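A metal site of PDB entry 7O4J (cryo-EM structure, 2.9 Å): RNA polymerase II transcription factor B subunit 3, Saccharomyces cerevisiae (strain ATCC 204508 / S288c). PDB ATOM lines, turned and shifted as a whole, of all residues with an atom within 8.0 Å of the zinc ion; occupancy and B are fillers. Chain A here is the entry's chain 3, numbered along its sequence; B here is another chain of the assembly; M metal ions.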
ATOM      1  N   MET A  15     -19.993  15.992 -19.759  1.00  0.00           N
ATOM      2  CA  MET A  15     -19.540  14.774 -20.419  1.00  0.00           C
ATOM      3  C   MET A  15     -18.336  14.202 -19.679  1.00  0.00           C
ATOM      4  O   MET A  15     -17.558  14.949 -19.081  1.00  0.00           O
ATOM      5  CB  MET A  15     -19.175  15.053 -21.870  1.00  0.00           C
ATOM      6  CG  MET A  15     -18.303  16.289 -22.069  1.00  0.00           C
ATOM      7  SD  MET A  15     -17.298  16.215 -23.556  1.00  0.00           S
ATOM      8  CE  MET A  15     -18.557  16.080 -24.817  1.00  0.00           C
ATOM      9  N   CYS A  16     -18.205  12.889 -19.728  1.00  0.00           N
ATOM     10  CA  CYS A  16     -17.056  12.240 -19.111  1.00  0.00           C
ATOM     11  C   CYS A  16     -15.783  12.691 -19.808  1.00  0.00           C
ATOM     12  O   CYS A  16     -15.662  12.551 -21.032  1.00  0.00           O
ATOM     13  CB  CYS A  16     -17.208  10.725 -19.212  1.00  0.00           C
ATOM     14  SG  CYS A  16     -15.867   9.773 -18.472  1.00  0.00           S
ATOM     15  N   PRO A  17     -14.802  13.241 -19.079  1.00  0.00           N
ATOM     16  CA  PRO A  17     -13.577  13.692 -19.745  1.00  0.00           C
ATOM     17  C   PRO A  17     -12.827  12.574 -20.454  1.00  0.00           C
ATOM     18  O   PRO A  17     -12.025  12.844 -21.356  1.00  0.00           O
ATOM     19  CB  PRO A  17     -12.748  14.282 -18.601  1.00  0.00           C
ATOM     20  CG  PRO A  17     -13.763  14.700 -17.591  1.00  0.00           C
ATOM     21  CD  PRO A  17     -14.845  13.677 -17.671  1.00  0.00           C
ATOM     22  N   ILE A  18     -13.055  11.318 -20.061  1.00  0.00           N
ATOM     23  CA  ILE A  18     -12.315  10.192 -20.614  1.00  0.00           C
ATOM     24  C   ILE A  18     -12.983   9.706 -21.893  1.00  0.00           C
ATOM     25  O   ILE A  18     -12.368   9.704 -22.970  1.00  0.00           O
ATOM     26  CB  ILE A  18     -12.189   9.058 -19.583  1.00  0.00           C
ATOM     27  CG1 ILE A  18     -11.635   9.591 -18.262  1.00  0.00           C
ATOM     28  CG2 ILE A  18     -11.296   7.950 -20.119  1.00  0.00           C
ATOM     29  CD1 ILE A  18     -10.436  10.509 -18.418  1.00  0.00           C
ATOM     30  N   CYS A  19     -14.240   9.290 -21.786  1.00  0.00           N
ATOM     31  CA  CYS A  19     -14.940   8.685 -22.910  1.00  0.00           C
ATOM     32  C   CYS A  19     -15.689   9.687 -23.751  1.00  0.00           C
ATOM     33  O   CYS A  19     -16.211   9.326 -24.804  1.00  0.00           O
ATOM     34  CB  CYS A  19     -15.909   7.617 -22.423  1.00  0.00           C
ATOM     35  SG  CYS A  19     -17.381   8.273 -21.654  1.00  0.00           S
ATOM     36  N   LYS A  20     -15.741  10.935 -23.315  1.00  0.00           N
ATOM     37  CA  LYS A  20     -16.458  11.979 -24.029  1.00  0.00           C
ATOM     38  C   LYS A  20     -17.885  11.568 -24.378  1.00  0.00           C
ATOM     39  O   LYS A  20     -18.350  11.779 -25.497  1.00  0.00           O
ATOM     40  CB  LYS A  20     -15.698  12.467 -25.261  1.00  0.00           C
ATOM     41  CG  LYS A  20     -14.984  13.780 -25.046  1.00  0.00           C
ATOM     42  CD  LYS A  20     -13.598  13.583 -24.494  1.00  0.00           C
ATOM     43  CE  LYS A  20     -12.893  14.921 -24.297  1.00  0.00           C
ATOM     44  NZ  LYS A  20     -11.414  14.775 -24.394  1.00  0.00           N
ATOM     45  N   THR A  21     -18.561  10.968 -23.412  1.00  0.00           N
ATOM     46  CA  THR A  21     -19.954  10.557 -23.540  1.00  0.00           C
ATOM     47  C   THR A  21     -20.840  11.716 -23.118  1.00  0.00           C
ATOM     48  O   THR A  21     -21.109  11.906 -21.937  1.00  0.00           O
ATOM     49  CB  THR A  21     -20.232   9.311 -22.699  1.00  0.00           C
ATOM     50  OG1 THR A  21     -21.543   8.817 -23.002  1.00  0.00           O
ATOM     51  CG2 THR A  21     -20.159   9.638 -21.214  1.00  0.00           C
ATOM     52  N   ASP A  22     -21.296  12.488 -24.102  1.00  0.00           N
ATOM     53  CA  ASP A  22     -22.162  13.631 -23.820  1.00  0.00           C
ATOM     54  C   ASP A  22     -23.508  13.160 -23.287  1.00  0.00           C
ATOM     55  O   ASP A  22     -23.998  12.071 -23.608  1.00  0.00           O
ATOM     56  CB  ASP A  22     -22.359  14.475 -25.078  1.00  0.00           C
ATOM     57  CG  ASP A  22     -22.922  15.843 -24.777  1.00  0.00           C
ATOM     58  OD1 ASP A  22     -23.979  15.920 -24.110  1.00  0.00           O
ATOM     59  OD2 ASP A  22     -22.317  16.847 -25.220  1.00  0.00           O
ATOM     60  N   VAL A  29     -26.506   8.663 -18.737  1.00  0.00           N
ATOM     61  CA  VAL A  29     -25.175   8.859 -18.180  1.00  0.00           C
ATOM     62  C   VAL A  29     -25.291   9.355 -16.745  1.00  0.00           C
ATOM     63  O   VAL A  29     -26.141  10.195 -16.417  1.00  0.00           O
ATOM     64  CB  VAL A  29     -24.367   9.846 -19.037  1.00  0.00           C
ATOM     65  CG1 VAL A  29     -25.018  11.222 -19.016  1.00  0.00           C
ATOM     66  CG2 VAL A  29     -22.930   9.927 -18.545  1.00  0.00           C
ATOM     67  N   LYS A  30     -24.438   8.820 -15.874  1.00  0.00           N
ATOM     68  CA  LYS A  30     -24.402   9.226 -14.467  1.00  0.00           C
ATOM     69  C   LYS A  30     -22.952   9.262 -14.019  1.00  0.00           C
ATOM     70  O   LYS A  30     -22.207   8.321 -14.272  1.00  0.00           O
ATOM     71  CB  LYS A  30     -25.228   8.262 -13.613  1.00  0.00           C
ATOM     72  CG  LYS A  30     -26.719   8.329 -13.893  1.00  0.00           C
ATOM     73  CD  LYS A  30     -27.517   7.480 -12.915  1.00  0.00           C
ATOM     74  CE  LYS A  30     -27.365   6.000 -13.206  1.00  0.00           C
ATOM     75  NZ  LYS A  30     -28.241   5.155 -12.345  1.00  0.00           N
ATOM     76  N   PHE A  31     -22.571  10.353 -13.349  1.00  0.00           N
ATOM     77  CA  PHE A  31     -21.189  10.562 -12.957  1.00  0.00           C
ATOM     78  C   PHE A  31     -20.993  10.231 -11.478  1.00  0.00           C
ATOM     79  O   PHE A  31     -21.930  10.213 -10.681  1.00  0.00           O
ATOM     80  CB  PHE A  31     -20.776  12.004 -13.224  1.00  0.00           C
ATOM     81  CG  PHE A  31     -20.834  12.388 -14.673  1.00  0.00           C
ATOM     82  CD1 PHE A  31     -22.034  12.779 -15.255  1.00  0.00           C
ATOM     83  CD2 PHE A  31     -19.689  12.369 -15.457  1.00  0.00           C
ATOM     84  CE1 PHE A  31     -22.087  13.138 -16.587  1.00  0.00           C
ATOM     85  CE2 PHE A  31     -19.742  12.729 -16.789  1.00  0.00           C
ATOM     86  CZ  PHE A  31     -20.942  13.104 -17.359  1.00  0.00           C
ATOM     87  N   ARG A  40     -14.243  13.531 -11.823  1.00  0.00           N
ATOM     88  CA  ARG A  40     -15.532  13.096 -12.347  1.00  0.00           C
ATOM     89  C   ARG A  40     -15.344  11.995 -13.383  1.00  0.00           C
ATOM     90  O   ARG A  40     -14.437  12.058 -14.222  1.00  0.00           O
ATOM     91  CB  ARG A  40     -16.271  14.279 -12.960  1.00  0.00           C
ATOM     92  CG  ARG A  40     -16.717  15.323 -11.948  1.00  0.00           C
ATOM     93  CD  ARG A  40     -17.463  16.464 -12.617  1.00  0.00           C
ATOM     94  NE  ARG A  40     -18.744  16.033 -13.170  1.00  0.00           N
ATOM     95  CZ  ARG A  40     -18.994  15.845 -14.461  1.00  0.00           C
ATOM     96  NH1 ARG A  40     -18.059  16.047 -15.380  1.00  0.00           N
ATOM     97  NH2 ARG A  40     -20.209  15.462 -14.845  1.00  0.00           N
ATOM     98  N   ILE A  41     -16.205  10.987 -13.329  1.00  0.00           N
ATOM     99  CA  ILE A  41     -16.143   9.869 -14.262  1.00  0.00           C
ATOM    100  C   ILE A  41     -17.531   9.241 -14.331  1.00  0.00           C
ATOM    101  O   ILE A  41     -18.179   9.033 -13.320  1.00  0.00           O
ATOM    102  CB  ILE A  41     -15.061   8.847 -13.849  1.00  0.00           C
ATOM    103  CG1 ILE A  41     -14.789   7.862 -14.994  1.00  0.00           C
ATOM    104  CG2 ILE A  41     -15.490   8.101 -12.594  1.00  0.00           C
ATOM    105  CD1 ILE A  41     -13.670   6.897 -14.703  1.00  0.00           C
ATOM    106  N   CYS A  42     -17.968   8.939 -15.551  1.00  0.00           N
ATOM    107  CA  CYS A  42     -19.264   8.315 -15.760  1.00  0.00           C
ATOM    108  C   CYS A  42     -19.227   6.848 -15.333  1.00  0.00           C
ATOM    109  O   CYS A  42     -18.178   6.208 -15.347  1.00  0.00           O
ATOM    110  CB  CYS A  42     -19.671   8.421 -17.234  1.00  0.00           C
ATOM    111  SG  CYS A  42     -18.807   7.268 -18.320  1.00  0.00           S
ATOM    112  N   GLU A  43     -20.395   6.332 -14.952  1.00  0.00           N
ATOM    113  CA  GLU A  43     -20.506   4.963 -14.453  1.00  0.00           C
ATOM    114  C   GLU A  43     -19.997   3.960 -15.491  1.00  0.00           C
ATOM    115  O   GLU A  43     -19.432   2.932 -15.132  1.00  0.00           O
ATOM    116  CB  GLU A  43     -21.949   4.648 -14.085  1.00  0.00           C
ATOM    117  CG  GLU A  43     -22.431   5.327 -12.812  1.00  0.00           C
ATOM    118  CD  GLU A  43     -23.859   4.971 -12.465  1.00  0.00           C
ATOM    119  OE1 GLU A  43     -24.506   4.263 -13.270  1.00  0.00           O
ATOM    120  OE2 GLU A  43     -24.336   5.399 -11.394  1.00  0.00           O
ATOM    121  N   SER A  44     -20.213   4.263 -16.773  1.00  0.00           N
ATOM    122  CA  SER A  44     -19.800   3.329 -17.824  1.00  0.00           C
ATOM    123  C   SER A  44     -18.289   3.088 -17.780  1.00  0.00           C
ATOM    124  O   SER A  44     -17.836   1.949 -17.911  1.00  0.00           O
ATOM    125  CB  SER A  44     -20.222   3.858 -19.183  1.00  0.00           C
ATOM    126  OG  SER A  44     -19.477   3.256 -20.222  1.00  0.00           O
ATOM    127  N   CYS A  45     -17.509   4.156 -17.606  1.00  0.00           N
ATOM    128  CA  CYS A  45     -16.061   3.996 -17.538  1.00  0.00           C
ATOM    129  C   CYS A  45     -15.632   3.272 -16.274  1.00  0.00           C
ATOM    130  O   CYS A  45     -14.633   2.530 -16.294  1.00  0.00           O
ATOM    131  CB  CYS A  45     -15.380   5.361 -17.608  1.00  0.00           C
ATOM    132  SG  CYS A  45     -15.360   6.091 -19.260  1.00  0.00           S
ATOM    133  N   VAL A  46     -16.360   3.455 -15.178  1.00  0.00           N
ATOM    134  CA  VAL A  46     -15.961   2.848 -13.908  1.00  0.00           C
ATOM    135  C   VAL A  46     -15.943   1.335 -14.032  1.00  0.00           C
ATOM    136  O   VAL A  46     -15.008   0.667 -13.587  1.00  0.00           O
ATOM    137  CB  VAL A  46     -16.904   3.313 -12.780  1.00  0.00           C
ATOM    138  CG1 VAL A  46     -16.573   2.593 -11.481  1.00  0.00           C
ATOM    139  CG2 VAL A  46     -16.808   4.820 -12.591  1.00  0.00           C
ATOM    140  N   ARG A  48     -15.669  -0.667 -16.714  1.00  0.00           N
ATOM    141  CA  ARG A  48     -14.706  -1.279 -17.637  1.00  0.00           C
ATOM    142  C   ARG A  48     -13.280  -1.097 -17.144  1.00  0.00           C
ATOM    143  O   ARG A  48     -12.416  -1.951 -17.389  1.00  0.00           O
ATOM    144  CB  ARG A  48     -14.873  -0.690 -19.035  1.00  0.00           C
ATOM    145  CG  ARG A  48     -14.354   0.732 -19.189  1.00  0.00           C
ATOM    146  CD  ARG A  48     -14.532   1.233 -20.621  1.00  0.00           C
ATOM    147  NE  ARG A  48     -14.241   2.658 -20.734  1.00  0.00           N
ATOM    148  CZ  ARG A  48     -13.026   3.174 -20.860  1.00  0.00           C
ATOM    149  NH1 ARG A  48     -11.961   2.374 -20.870  1.00  0.00           N
ATOM    150  NH2 ARG A  48     -12.866   4.479 -20.955  1.00  0.00           N
ATOM    151  N   ILE A  49     -12.996  -0.001 -16.439  1.00  0.00           N
ATOM    152  CA  ILE A  49     -11.628   0.279 -16.036  1.00  0.00           C
ATOM    153  C   ILE A  49     -11.279  -0.376 -14.699  1.00  0.00           C
ATOM    154  O   ILE A  49     -10.112  -0.680 -14.439  1.00  0.00           O
ATOM    155  CB  ILE A  49     -11.378   1.796 -15.975  1.00  0.00           C
ATOM    156  CG1 ILE A  49     -11.523   2.411 -17.370  1.00  0.00           C
ATOM    157  CG2 ILE A  49     -10.006   2.099 -15.389  1.00  0.00           C
ATOM    158  CD1 ILE A  49     -11.470   3.925 -17.393  1.00  0.00           C
ATOM    159  N   LYS B 110     -17.995   3.242 -28.671  1.00  0.00           N
ATOM    160  CA  LYS B 110     -17.973   3.028 -27.229  1.00  0.00           C
ATOM    161  C   LYS B 110     -17.983   1.543 -26.896  1.00  0.00           C
ATOM    162  O   LYS B 110     -17.232   1.095 -26.014  1.00  0.00           O
ATOM    163  CB  LYS B 110     -19.178   3.719 -26.583  1.00  0.00           C
ATOM    164  CG  LYS B 110     -19.081   5.244 -26.571  1.00  0.00           C
ATOM    165  CD  LYS B 110     -20.373   5.876 -26.094  1.00  0.00           C
ATOM    166  CE  LYS B 110     -20.638   5.570 -24.624  1.00  0.00           C
ATOM    167  NZ  LYS B 110     -21.851   6.277 -24.126  1.00  0.00           N
ATOM    168  N   LEU B 113     -14.631   0.118 -27.554  1.00  0.00           N
ATOM    169  CA  LEU B 113     -13.747   0.434 -26.440  1.00  0.00           C
ATOM    170  C   LEU B 113     -13.942  -0.549 -25.291  1.00  0.00           C
ATOM    171  O   LEU B 113     -12.979  -1.013 -24.687  1.00  0.00           O
ATOM    172  CB  LEU B 113     -14.001   1.868 -25.965  1.00  0.00           C
ATOM    173  CG  LEU B 113     -13.228   2.328 -24.731  1.00  0.00           C
ATOM    174  CD1 LEU B 113     -11.741   2.084 -24.893  1.00  0.00           C
ATOM    175  CD2 LEU B 113     -13.501   3.810 -24.463  1.00  0.00           C
ATOM    176  N   LEU B 172     -12.441   7.792 -30.118  1.00  0.00           N
ATOM    177  CA  LEU B 172     -13.628   8.408 -29.557  1.00  0.00           C
ATOM    178  C   LEU B 172     -13.386   9.873 -29.231  1.00  0.00           C
ATOM    179  O   LEU B 172     -14.250  10.732 -29.465  1.00  0.00           O
ATOM    180  CB  LEU B 172     -14.089   7.653 -28.317  1.00  0.00           C
ATOM    181  CG  LEU B 172     -15.541   7.867 -27.874  1.00  0.00           C
ATOM    182  CD1 LEU B 172     -16.514   7.569 -29.002  1.00  0.00           C
ATOM    183  CD2 LEU B 172     -15.852   7.008 -26.665  1.00  0.00           C
HETATM  184 ZN    ZN M   1     -16.851   7.877 -19.421  1.00  0.00          ZN
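The zinc ion is bound by the side-chain sulfur of Cys 42, the side-chain sulfur of Cys 19, the side-chain sulfur of Cys 45 and the side-chain sulfur of Cys 16.
The side-chain sulfur of Cys 16 lies close to the backbone NH of Ile 18, 3.6 Å away. SG of Cys 45 lies close to NH2 of Arg 48, at 3.4 Å. N of Thr 21 lies close to SG of Cys 19 (3.4 Å). N of Ser 44 lies close to SG of Cys 42 (3.7 Å).
Of the 23 residues printed, 4 come within 4 Å of the zinc ion.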
